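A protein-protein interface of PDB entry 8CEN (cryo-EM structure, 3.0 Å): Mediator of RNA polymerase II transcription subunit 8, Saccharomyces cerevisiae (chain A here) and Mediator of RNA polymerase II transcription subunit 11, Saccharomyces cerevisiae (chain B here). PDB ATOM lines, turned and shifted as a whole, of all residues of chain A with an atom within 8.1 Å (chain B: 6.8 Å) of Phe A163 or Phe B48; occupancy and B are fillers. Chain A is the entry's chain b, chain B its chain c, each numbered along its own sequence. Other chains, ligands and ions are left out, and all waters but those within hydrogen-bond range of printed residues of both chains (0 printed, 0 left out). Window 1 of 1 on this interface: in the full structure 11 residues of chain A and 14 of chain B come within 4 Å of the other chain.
The side-chain carboxylate of Glu A166 lies close to the backbone carbonyl oxygen of Lys B53.
O of Thr A162 sits close to OD1 of Asn A165. O of Trp A158 lies within hydrogen-bond range of OG1 of Thr A162, at 2.7 Å.
Among the printed residues, pairs that only touch across the chains: Ile A155 with Leu B37 (3.6 Å), Trp A158 with Lys B45 (3.5 Å), Trp A158 with Phe B48 (3.6 Å), Ala A159 with Phe B34 (3.6 Å), Ala A159 with Phe B48 (3.99 Å), Thr A162 with Glu B49 (3.3 Å), Phe A163 with Phe B48 (3.7 Å), Phe A163 with Val B52 (3.6 Å) and Glu A166 with Tyr B56 (3.6 Å).
Of the printed residues of chain B, Trp A158 touches Lys B45 (3.5 Å) and Phe B48 (3.6 Å). Asn A165 touches none of the printed residues of chain B. Val B30 touches none of the printed residues of chain A. Of the printed residues of chain A, Leu B37 touches Ile A155. Printed residues of chain A within 4 Å of Phe B48: Trp A158 (3.6 Å), Ala A159 (3.99 Å) and Phe A163 (3.7 Å). The nearest printed residue of chain A that does not touch Phe B48 is Thr A162 (4.7 Å).
Of the 18 printed residues of chain B, 8 touch a printed residue of chain A. Hydrophobic or aromatic side chains of chain B within 4 Å of the printed part of chain A: Phe B34, Leu B37, Phe B48, Val B52 and Tyr B56. Hydrophobic or aromatic side chains of chain A within 4 Å of the printed part of chain B: Ile A155, Trp A158, Ala A159 and Phe A163. Among the printed residues, no Asp or Glu carboxylate lies within 4 Å of a Lys or Arg side-chain nitrogen of the other chain.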
ATOM      1  N   ILE A 155      -9.972   1.547 -29.112  1.00  0.00           N
ATOM      2  CA  ILE A 155     -11.096   0.930 -28.406  1.00  0.00           C
ATOM      3  C   ILE A 155     -11.108   1.342 -26.934  1.00  0.00           C
ATOM      4  O   ILE A 155     -12.172   1.623 -26.363  1.00  0.00           O
ATOM      5  CB  ILE A 155     -11.063  -0.603 -28.574  1.00  0.00           C
ATOM      6  CG1 ILE A 155     -11.236  -0.990 -30.042  1.00  0.00           C
ATOM      7  CG2 ILE A 155     -12.158  -1.258 -27.779  1.00  0.00           C
ATOM      8  CD1 ILE A 155     -10.957  -2.452 -30.324  1.00  0.00           C
ATOM      9  N   THR A 156      -9.931   1.397 -26.300  1.00  0.00           N
ATOM     10  CA  THR A 156      -9.867   1.860 -24.911  1.00  0.00           C
ATOM     11  C   THR A 156     -10.293   3.321 -24.785  1.00  0.00           C
ATOM     12  O   THR A 156     -10.956   3.700 -23.810  1.00  0.00           O
ATOM     13  CB  THR A 156      -8.464   1.676 -24.330  1.00  0.00           C
ATOM     14  OG1 THR A 156      -7.544   2.545 -25.000  1.00  0.00           O
ATOM     15  CG2 THR A 156      -8.007   0.236 -24.440  1.00  0.00           C
ATOM     16  N   ASN A 157      -9.912   4.157 -25.756  1.00  0.00           N
ATOM     17  CA  ASN A 157     -10.338   5.553 -25.751  1.00  0.00           C
ATOM     18  C   ASN A 157     -11.850   5.671 -25.903  1.00  0.00           C
ATOM     19  O   ASN A 157     -12.485   6.508 -25.245  1.00  0.00           O
ATOM     20  CB  ASN A 157      -9.626   6.320 -26.864  1.00  0.00           C
ATOM     21  CG  ASN A 157      -9.507   7.801 -26.567  1.00  0.00           C
ATOM     22  OD1 ASN A 157     -10.084   8.300 -25.601  1.00  0.00           O
ATOM     23  ND2 ASN A 157      -8.755   8.512 -27.398  1.00  0.00           N
ATOM     24  N   TRP A 158     -12.442   4.835 -26.766  1.00  0.00           N
ATOM     25  CA  TRP A 158     -13.897   4.817 -26.893  1.00  0.00           C
ATOM     26  C   TRP A 158     -14.554   4.405 -25.582  1.00  0.00           C
ATOM     27  O   TRP A 158     -15.575   4.975 -25.182  1.00  0.00           O
ATOM     28  CB  TRP A 158     -14.353   3.845 -27.975  1.00  0.00           C
ATOM     29  CG  TRP A 158     -15.838   3.895 -28.100  1.00  0.00           C
ATOM     30  CD1 TRP A 158     -16.582   4.944 -28.551  1.00  0.00           C
ATOM     31  CD2 TRP A 158     -16.772   2.950 -27.565  1.00  0.00           C
ATOM     32  NE1 TRP A 158     -17.921   4.660 -28.444  1.00  0.00           N
ATOM     33  CE2 TRP A 158     -18.064   3.445 -27.826  1.00  0.00           C
ATOM     34  CE3 TRP A 158     -16.640   1.712 -26.931  1.00  0.00           C
ATOM     35  CZ2 TRP A 158     -19.216   2.747 -27.477  1.00  0.00           C
ATOM     36  CZ3 TRP A 158     -17.783   1.023 -26.580  1.00  0.00           C
ATOM     37  CH2 TRP A 158     -19.056   1.540 -26.857  1.00  0.00           C
ATOM     38  N   ALA A 159     -13.996   3.390 -24.917  1.00  0.00           N
ATOM     39  CA  ALA A 159     -14.573   2.915 -23.664  1.00  0.00           C
ATOM     40  C   ALA A 159     -14.497   3.981 -22.579  1.00  0.00           C
ATOM     41  O   ALA A 159     -15.452   4.175 -21.816  1.00  0.00           O
ATOM     42  CB  ALA A 159     -13.868   1.637 -23.212  1.00  0.00           C
ATOM     43  N   ARG A 160     -13.382   4.710 -22.513  1.00  0.00           N
ATOM     44  CA  ARG A 160     -13.267   5.723 -21.472  1.00  0.00           C
ATOM     45  C   ARG A 160     -14.101   6.966 -21.777  1.00  0.00           C
ATOM     46  O   ARG A 160     -14.622   7.588 -20.844  1.00  0.00           O
ATOM     47  CB  ARG A 160     -11.797   6.077 -21.223  1.00  0.00           C
ATOM     48  CG  ARG A 160     -11.090   6.895 -22.284  1.00  0.00           C
ATOM     49  CD  ARG A 160      -9.663   7.170 -21.832  1.00  0.00           C
ATOM     50  NE  ARG A 160      -8.947   8.081 -22.715  1.00  0.00           N
ATOM     51  CZ  ARG A 160      -7.719   8.528 -22.487  1.00  0.00           C
ATOM     52  NH1 ARG A 160      -7.040   8.163 -21.411  1.00  0.00           N
ATOM     53  NH2 ARG A 160      -7.159   9.362 -23.357  1.00  0.00           N
ATOM     54  N   THR A 161     -14.299   7.326 -23.050  1.00  0.00           N
ATOM     55  CA  THR A 161     -15.223   8.431 -23.306  1.00  0.00           C
ATOM     56  C   THR A 161     -16.679   7.998 -23.142  1.00  0.00           C
ATOM     57  O   THR A 161     -17.533   8.828 -22.802  1.00  0.00           O
ATOM     58  CB  THR A 161     -14.979   9.057 -24.688  1.00  0.00           C
ATOM     59  OG1 THR A 161     -15.767  10.247 -24.816  1.00  0.00           O
ATOM     60  CG2 THR A 161     -15.338   8.113 -25.819  1.00  0.00           C
ATOM     61  N   THR A 162     -16.975   6.706 -23.339  1.00  0.00           N
ATOM     62  CA  THR A 162     -18.289   6.179 -22.989  1.00  0.00           C
ATOM     63  C   THR A 162     -18.528   6.276 -21.489  1.00  0.00           C
ATOM     64  O   THR A 162     -19.614   6.673 -21.047  1.00  0.00           O
ATOM     65  CB  THR A 162     -18.416   4.731 -23.465  1.00  0.00           C
ATOM     66  OG1 THR A 162     -18.240   4.680 -24.886  1.00  0.00           O
ATOM     67  CG2 THR A 162     -19.782   4.164 -23.115  1.00  0.00           C
ATOM     68  N   PHE A 163     -17.508   5.940 -20.693  1.00  0.00           N
ATOM     69  CA  PHE A 163     -17.580   6.137 -19.247  1.00  0.00           C
ATOM     70  C   PHE A 163     -17.781   7.602 -18.895  1.00  0.00           C
ATOM     71  O   PHE A 163     -18.563   7.926 -17.994  1.00  0.00           O
ATOM     72  CB  PHE A 163     -16.311   5.622 -18.574  1.00  0.00           C
ATOM     73  CG  PHE A 163     -16.157   4.137 -18.610  1.00  0.00           C
ATOM     74  CD1 PHE A 163     -17.223   3.310 -18.924  1.00  0.00           C
ATOM     75  CD2 PHE A 163     -14.933   3.567 -18.333  1.00  0.00           C
ATOM     76  CE1 PHE A 163     -17.065   1.943 -18.953  1.00  0.00           C
ATOM     77  CE2 PHE A 163     -14.775   2.211 -18.365  1.00  0.00           C
ATOM     78  CZ  PHE A 163     -15.838   1.393 -18.673  1.00  0.00           C
ATOM     79  N   ARG A 164     -17.080   8.498 -19.594  1.00  0.00           N
ATOM     80  CA  ARG A 164     -17.173   9.924 -19.298  1.00  0.00           C
ATOM     81  C   ARG A 164     -18.578  10.456 -19.559  1.00  0.00           C
ATOM     82  O   ARG A 164     -19.155  11.150 -18.712  1.00  0.00           O
ATOM     83  CB  ARG A 164     -16.138  10.691 -20.121  1.00  0.00           C
ATOM     84  CG  ARG A 164     -16.144  12.192 -19.899  1.00  0.00           C
ATOM     85  CD  ARG A 164     -15.001  12.853 -20.649  1.00  0.00           C
ATOM     86  NE  ARG A 164     -13.743  12.745 -19.920  1.00  0.00           N
ATOM     87  CZ  ARG A 164     -12.781  11.879 -20.210  1.00  0.00           C
ATOM     88  NH1 ARG A 164     -12.894  11.033 -21.221  1.00  0.00           N
ATOM     89  NH2 ARG A 164     -11.679  11.859 -19.466  1.00  0.00           N
ATOM     90  N   ASN A 165     -19.166  10.109 -20.709  1.00  0.00           N
ATOM     91  CA  ASN A 165     -20.506  10.616 -20.999  1.00  0.00           C
ATOM     92  C   ASN A 165     -21.574   9.934 -20.145  1.00  0.00           C
ATOM     93  O   ASN A 165     -22.543  10.588 -19.740  1.00  0.00           O
ATOM     94  CB  ASN A 165     -20.824  10.508 -22.499  1.00  0.00           C
ATOM     95  CG  ASN A 165     -20.779   9.083 -23.033  1.00  0.00           C
ATOM     96  OD1 ASN A 165     -21.495   8.194 -22.572  1.00  0.00           O
ATOM     97  ND2 ASN A 165     -19.947   8.874 -24.046  1.00  0.00           N
ATOM     98  N   GLU A 166     -21.407   8.644 -19.829  1.00  0.00           N
ATOM     99  CA  GLU A 166     -22.372   7.976 -18.962  1.00  0.00           C
ATOM    100  C   GLU A 166     -22.308   8.519 -17.538  1.00  0.00           C
ATOM    101  O   GLU A 166     -23.339   8.635 -16.864  1.00  0.00           O
ATOM    102  CB  GLU A 166     -22.133   6.464 -18.980  1.00  0.00           C
ATOM    103  CG  GLU A 166     -23.114   5.651 -18.142  1.00  0.00           C
ATOM    104  CD  GLU A 166     -24.543   5.716 -18.657  1.00  0.00           C
ATOM    105  OE1 GLU A 166     -24.741   5.948 -19.869  1.00  0.00           O
ATOM    106  OE2 GLU A 166     -25.472   5.532 -17.845  1.00  0.00           O
ATOM    107  N   TYR A 167     -21.109   8.869 -17.066  1.00  0.00           N
ATOM    108  CA  TYR A 167     -20.972   9.454 -15.738  1.00  0.00           C
ATOM    109  C   TYR A 167     -21.492  10.887 -15.712  1.00  0.00           C
ATOM    110  O   TYR A 167     -22.057  11.328 -14.705  1.00  0.00           O
ATOM    111  CB  TYR A 167     -19.510   9.390 -15.297  1.00  0.00           C
ATOM    112  CG  TYR A 167     -19.143  10.327 -14.170  1.00  0.00           C
ATOM    113  CD1 TYR A 167     -19.503  10.041 -12.862  1.00  0.00           C
ATOM    114  CD2 TYR A 167     -18.414  11.486 -14.411  1.00  0.00           C
ATOM    115  CE1 TYR A 167     -19.167  10.889 -11.824  1.00  0.00           C
ATOM    116  CE2 TYR A 167     -18.072  12.341 -13.379  1.00  0.00           C
ATOM    117  CZ  TYR A 167     -18.451  12.036 -12.089  1.00  0.00           C
ATOM    118  OH  TYR A 167     -18.113  12.882 -11.057  1.00  0.00           O
ATOM    119  N   GLY A 168     -21.314  11.627 -16.810  1.00  0.00           N
ATOM    120  CA  GLY A 168     -21.875  12.964 -16.893  1.00  0.00           C
ATOM    121  C   GLY A 168     -23.378  12.989 -17.071  1.00  0.00           C
ATOM    122  O   GLY A 168     -24.004  14.018 -16.794  1.00  0.00           O
ATOM    123  N   LYS A 169     -23.964  11.888 -17.549  1.00  0.00           N
ATOM    124  CA  LYS A 169     -25.418  11.806 -17.666  1.00  0.00           C
ATOM    125  C   LYS A 169     -26.097  11.881 -16.302  1.00  0.00           C
ATOM    126  O   LYS A 169     -27.095  12.592 -16.136  1.00  0.00           O
ATOM    127  CB  LYS A 169     -25.807  10.515 -18.390  1.00  0.00           C
ATOM    128  CG  LYS A 169     -27.295  10.196 -18.359  1.00  0.00           C
ATOM    129  CD  LYS A 169     -27.583   8.810 -18.915  1.00  0.00           C
ATOM    130  CE  LYS A 169     -26.985   8.627 -20.301  1.00  0.00           C
ATOM    131  NZ  LYS A 169     -27.501   9.637 -21.267  1.00  0.00           N
ATOM    132  N   GLN B  29     -20.137  -8.422 -15.420  1.00  0.00           N
ATOM    133  CA  GLN B  29     -20.463  -8.531 -16.835  1.00  0.00           C
ATOM    134  C   GLN B  29     -19.768  -7.443 -17.644  1.00  0.00           C
ATOM    135  O   GLN B  29     -19.314  -7.699 -18.761  1.00  0.00           O
ATOM    136  CB  GLN B  29     -21.976  -8.476 -17.033  1.00  0.00           C
ATOM    137  CG  GLN B  29     -22.423  -8.924 -18.414  1.00  0.00           C
ATOM    138  CD  GLN B  29     -22.173 -10.401 -18.651  1.00  0.00           C
ATOM    139  OE1 GLN B  29     -22.402 -11.230 -17.770  1.00  0.00           O
ATOM    140  NE2 GLN B  29     -21.699 -10.738 -19.845  1.00  0.00           N
ATOM    141  N   VAL B  30     -19.649  -6.236 -17.086  1.00  0.00           N
ATOM    142  CA  VAL B  30     -18.970  -5.147 -17.786  1.00  0.00           C
ATOM    143  C   VAL B  30     -17.490  -5.472 -17.973  1.00  0.00           C
ATOM    144  O   VAL B  30     -16.935  -5.297 -19.067  1.00  0.00           O
ATOM    145  CB  VAL B  30     -19.179  -3.818 -17.036  1.00  0.00           C
ATOM    146  CG1 VAL B  30     -18.143  -2.789 -17.441  1.00  0.00           C
ATOM    147  CG2 VAL B  30     -20.570  -3.272 -17.306  1.00  0.00           C
ATOM    148  N   THR B  31     -16.836  -5.979 -16.918  1.00  0.00           N
ATOM    149  CA  THR B  31     -15.439  -6.392 -17.042  1.00  0.00           C
ATOM    150  C   THR B  31     -15.271  -7.562 -18.007  1.00  0.00           C
ATOM    151  O   THR B  31     -14.288  -7.601 -18.755  1.00  0.00           O
ATOM    152  CB  THR B  31     -14.854  -6.751 -15.674  1.00  0.00           C
ATOM    153  OG1 THR B  31     -15.587  -7.844 -15.104  1.00  0.00           O
ATOM    154  CG2 THR B  31     -14.881  -5.553 -14.736  1.00  0.00           C
ATOM    155  N   ILE B  33     -17.239  -8.230 -20.721  1.00  0.00           N
ATOM    156  CA  ILE B  33     -17.450  -7.728 -22.076  1.00  0.00           C
ATOM    157  C   ILE B  33     -16.255  -6.900 -22.528  1.00  0.00           C
ATOM    158  O   ILE B  33     -15.791  -7.029 -23.673  1.00  0.00           O
ATOM    159  CB  ILE B  33     -18.762  -6.923 -22.155  1.00  0.00           C
ATOM    160  CG1 ILE B  33     -19.983  -7.781 -21.800  1.00  0.00           C
ATOM    161  CG2 ILE B  33     -18.944  -6.347 -23.533  1.00  0.00           C
ATOM    162  CD1 ILE B  33     -20.302  -8.885 -22.762  1.00  0.00           C
ATOM    163  N   PHE B  34     -15.716  -6.065 -21.625  1.00  0.00           N
ATOM    164  CA  PHE B  34     -14.457  -5.381 -21.901  1.00  0.00           C
ATOM    165  C   PHE B  34     -13.336  -6.377 -22.160  1.00  0.00           C
ATOM    166  O   PHE B  34     -12.452  -6.110 -22.980  1.00  0.00           O
ATOM    167  CB  PHE B  34     -14.078  -4.456 -20.743  1.00  0.00           C
ATOM    168  CG  PHE B  34     -13.009  -3.458 -21.093  1.00  0.00           C
ATOM    169  CD1 PHE B  34     -13.273  -2.419 -21.968  1.00  0.00           C
ATOM    170  CD2 PHE B  34     -11.736  -3.568 -20.560  1.00  0.00           C
ATOM    171  CE1 PHE B  34     -12.293  -1.503 -22.298  1.00  0.00           C
ATOM    172  CE2 PHE B  34     -10.749  -2.655 -20.885  1.00  0.00           C
ATOM    173  CZ  PHE B  34     -11.028  -1.622 -21.757  1.00  0.00           C
ATOM    174  N   GLY B  35     -13.387  -7.541 -21.505  1.00  0.00           N
ATOM    175  CA  GLY B  35     -12.398  -8.575 -21.758  1.00  0.00           C
ATOM    176  C   GLY B  35     -12.396  -9.067 -23.193  1.00  0.00           C
ATOM    177  O   GLY B  35     -11.350  -9.079 -23.850  1.00  0.00           O
ATOM    178  N   LEU B  37     -13.778  -7.623 -25.804  1.00  0.00           N
ATOM    179  CA  LEU B  37     -13.529  -6.578 -26.795  1.00  0.00           C
ATOM    180  C   LEU B  37     -12.094  -6.058 -26.753  1.00  0.00           C
ATOM    181  O   LEU B  37     -11.650  -5.442 -27.727  1.00  0.00           O
ATOM    182  CB  LEU B  37     -14.525  -5.417 -26.666  1.00  0.00           C
ATOM    183  CG  LEU B  37     -14.745  -4.551 -25.429  1.00  0.00           C
ATOM    184  CD1 LEU B  37     -13.784  -3.391 -25.350  1.00  0.00           C
ATOM    185  CD2 LEU B  37     -16.174  -4.047 -25.409  1.00  0.00           C
ATOM    186  N   VAL B  44     -19.924  -6.924 -29.983  1.00  0.00           N
ATOM    187  CA  VAL B  44     -20.543  -6.899 -28.663  1.00  0.00           C
ATOM    188  C   VAL B  44     -20.438  -5.490 -28.051  1.00  0.00           C
ATOM    189  O   VAL B  44     -20.871  -5.244 -26.916  1.00  0.00           O
ATOM    190  CB  VAL B  44     -19.900  -8.031 -27.819  1.00  0.00           C
ATOM    191  CG1 VAL B  44     -20.360  -8.140 -26.361  1.00  0.00           C
ATOM    192  CG2 VAL B  44     -20.081  -9.371 -28.527  1.00  0.00           C
ATOM    193  N   LYS B  45     -19.952  -4.533 -28.844  1.00  0.00           N
ATOM    194  CA  LYS B  45     -19.808  -3.138 -28.424  1.00  0.00           C
ATOM    195  C   LYS B  45     -21.105  -2.470 -27.943  1.00  0.00           C
ATOM    196  O   LYS B  45     -21.065  -1.799 -26.890  1.00  0.00           O
ATOM    197  CB  LYS B  45     -19.149  -2.378 -29.583  1.00  0.00           C
ATOM    198  CG  LYS B  45     -18.602  -1.020 -29.263  1.00  0.00           C
ATOM    199  CD  LYS B  45     -18.038  -0.351 -30.506  1.00  0.00           C
ATOM    200  CE  LYS B  45     -16.763  -1.039 -30.974  1.00  0.00           C
ATOM    201  NZ  LYS B  45     -16.154  -0.354 -32.149  1.00  0.00           N
ATOM    202  N   PRO B  46     -22.261  -2.581 -28.628  1.00  0.00           N
ATOM    203  CA  PRO B  46     -23.491  -2.039 -28.020  1.00  0.00           C
ATOM    204  C   PRO B  46     -23.895  -2.737 -26.734  1.00  0.00           C
ATOM    205  O   PRO B  46     -24.503  -2.100 -25.865  1.00  0.00           O
ATOM    206  CB  PRO B  46     -24.545  -2.229 -29.120  1.00  0.00           C
ATOM    207  CG  PRO B  46     -24.042  -3.339 -29.932  1.00  0.00           C
ATOM    208  CD  PRO B  46     -22.561  -3.145 -29.962  1.00  0.00           C
ATOM    209  N   GLN B  47     -23.577  -4.026 -26.584  1.00  0.00           N
ATOM    210  CA  GLN B  47     -23.830  -4.703 -25.315  1.00  0.00           C
ATOM    211  C   GLN B  47     -22.965  -4.125 -24.203  1.00  0.00           C
ATOM    212  O   GLN B  47     -23.424  -3.996 -23.061  1.00  0.00           O
ATOM    213  CB  GLN B  47     -23.600  -6.209 -25.451  1.00  0.00           C
ATOM    214  CG  GLN B  47     -24.738  -6.972 -26.120  1.00  0.00           C
ATOM    215  CD  GLN B  47     -24.830  -6.717 -27.611  1.00  0.00           C
ATOM    216  OE1 GLN B  47     -23.899  -7.008 -28.361  1.00  0.00           O
ATOM    217  NE2 GLN B  47     -25.958  -6.172 -28.049  1.00  0.00           N
ATOM    218  N   PHE B  48     -21.715  -3.769 -24.519  1.00  0.00           N
ATOM    219  CA  PHE B  48     -20.861  -3.084 -23.547  1.00  0.00           C
ATOM    220  C   PHE B  48     -21.471  -1.754 -23.131  1.00  0.00           C
ATOM    221  O   PHE B  48     -21.524  -1.423 -21.936  1.00  0.00           O
ATOM    222  CB  PHE B  48     -19.465  -2.862 -24.133  1.00  0.00           C
ATOM    223  CG  PHE B  48     -18.552  -2.053 -23.249  1.00  0.00           C
ATOM    224  CD1 PHE B  48     -17.890  -2.652 -22.190  1.00  0.00           C
ATOM    225  CD2 PHE B  48     -18.329  -0.705 -23.496  1.00  0.00           C
ATOM    226  CE1 PHE B  48     -17.044  -1.920 -21.377  1.00  0.00           C
ATOM    227  CE2 PHE B  48     -17.485   0.032 -22.686  1.00  0.00           C
ATOM    228  CZ  PHE B  48     -16.840  -0.577 -21.627  1.00  0.00           C
ATOM    229  N   GLU B  49     -21.941  -0.981 -24.117  1.00  0.00           N
ATOM    230  CA  GLU B  49     -22.555   0.314 -23.824  1.00  0.00           C
ATOM    231  C   GLU B  49     -23.798   0.156 -22.951  1.00  0.00           C
ATOM    232  O   GLU B  49     -23.969   0.883 -21.962  1.00  0.00           O
ATOM    233  CB  GLU B  49     -22.903   1.029 -25.130  1.00  0.00           C
ATOM    234  CG  GLU B  49     -23.874   2.192 -24.981  1.00  0.00           C
ATOM    235  CD  GLU B  49     -23.260   3.388 -24.280  1.00  0.00           C
ATOM    236  OE1 GLU B  49     -22.569   4.182 -24.953  1.00  0.00           O
ATOM    237  OE2 GLU B  49     -23.472   3.539 -23.058  1.00  0.00           O
ATOM    238  N   ASN B  50     -24.649  -0.821 -23.277  1.00  0.00           N
ATOM    239  CA  ASN B  50     -25.870  -1.046 -22.510  1.00  0.00           C
ATOM    240  C   ASN B  50     -25.568  -1.527 -21.097  1.00  0.00           C
ATOM    241  O   ASN B  50     -26.249  -1.131 -20.146  1.00  0.00           O
ATOM    242  CB  ASN B  50     -26.766  -2.049 -23.235  1.00  0.00           C
ATOM    243  CG  ASN B  50     -27.303  -1.509 -24.542  1.00  0.00           C
ATOM    244  OD1 ASN B  50     -27.079  -0.348 -24.886  1.00  0.00           O
ATOM    245  ND2 ASN B  50     -28.016  -2.350 -25.283  1.00  0.00           N
ATOM    246  N   HIS B  51     -24.551  -2.379 -20.937  1.00  0.00           N
ATOM    247  CA  HIS B  51     -24.219  -2.886 -19.610  1.00  0.00           C
ATOM    248  C   HIS B  51     -23.651  -1.788 -18.719  1.00  0.00           C
ATOM    249  O   HIS B  51     -24.004  -1.702 -17.536  1.00  0.00           O
ATOM    250  CB  HIS B  51     -23.245  -4.056 -19.727  1.00  0.00           C
ATOM    251  CG  HIS B  51     -23.915  -5.363 -20.009  1.00  0.00           C
ATOM    252  ND1 HIS B  51     -23.987  -5.903 -21.275  1.00  0.00           N
ATOM    253  CD2 HIS B  51     -24.558  -6.230 -19.192  1.00  0.00           C
ATOM    254  CE1 HIS B  51     -24.638  -7.052 -21.224  1.00  0.00           C
ATOM    255  NE2 HIS B  51     -24.996  -7.273 -19.973  1.00  0.00           N
ATOM    256  N   VAL B  52     -22.792  -0.924 -19.271  1.00  0.00           N
ATOM    257  CA  VAL B  52     -22.277   0.200 -18.489  1.00  0.00           C
ATOM    258  C   VAL B  52     -23.405   1.165 -18.129  1.00  0.00           C
ATOM    259  O   VAL B  52     -23.484   1.662 -16.994  1.00  0.00           O
ATOM    260  CB  VAL B  52     -21.137   0.900 -19.251  1.00  0.00           C
ATOM    261  CG1 VAL B  52     -20.679   2.149 -18.517  1.00  0.00           C
ATOM    262  CG2 VAL B  52     -19.974  -0.056 -19.424  1.00  0.00           C
ATOM    263  N   LYS B  53     -24.316   1.412 -19.080  1.00  0.00           N
ATOM    264  CA  LYS B  53     -25.446   2.300 -18.825  1.00  0.00           C
ATOM    265  C   LYS B  53     -26.356   1.749 -17.730  1.00  0.00           C
ATOM    266  O   LYS B  53     -26.794   2.496 -16.845  1.00  0.00           O
ATOM    267  CB  LYS B  53     -26.230   2.525 -20.120  1.00  0.00           C
ATOM    268  CG  LYS B  53     -27.384   3.516 -20.013  1.00  0.00           C
ATOM    269  CD  LYS B  53     -28.734   2.815 -19.987  1.00  0.00           C
ATOM    270  CE  LYS B  53     -29.056   2.176 -21.325  1.00  0.00           C
ATOM    271  NZ  LYS B  53     -30.382   1.500 -21.293  1.00  0.00           N
ATOM    272  N   TYR B  56     -24.695   2.074 -14.286  1.00  0.00           N
ATOM    273  CA  TYR B  56     -24.748   3.420 -13.723  1.00  0.00           C
ATOM    274  C   TYR B  56     -26.162   3.838 -13.333  1.00  0.00           C
ATOM    275  O   TYR B  56     -26.336   4.514 -12.311  1.00  0.00           O
ATOM    276  CB  TYR B  56     -24.133   4.428 -14.691  1.00  0.00           C
ATOM    277  CG  TYR B  56     -22.653   4.636 -14.465  1.00  0.00           C
ATOM    278  CD1 TYR B  56     -22.204   5.494 -13.469  1.00  0.00           C
ATOM    279  CD2 TYR B  56     -21.707   3.976 -15.237  1.00  0.00           C
ATOM    280  CE1 TYR B  56     -20.854   5.693 -13.249  1.00  0.00           C
ATOM    281  CE2 TYR B  56     -20.352   4.169 -15.025  1.00  0.00           C
ATOM    282  CZ  TYR B  56     -19.933   5.028 -14.029  1.00  0.00           C
ATOM    283  OH  TYR B  56     -18.589   5.225 -13.813  1.00  0.00           O
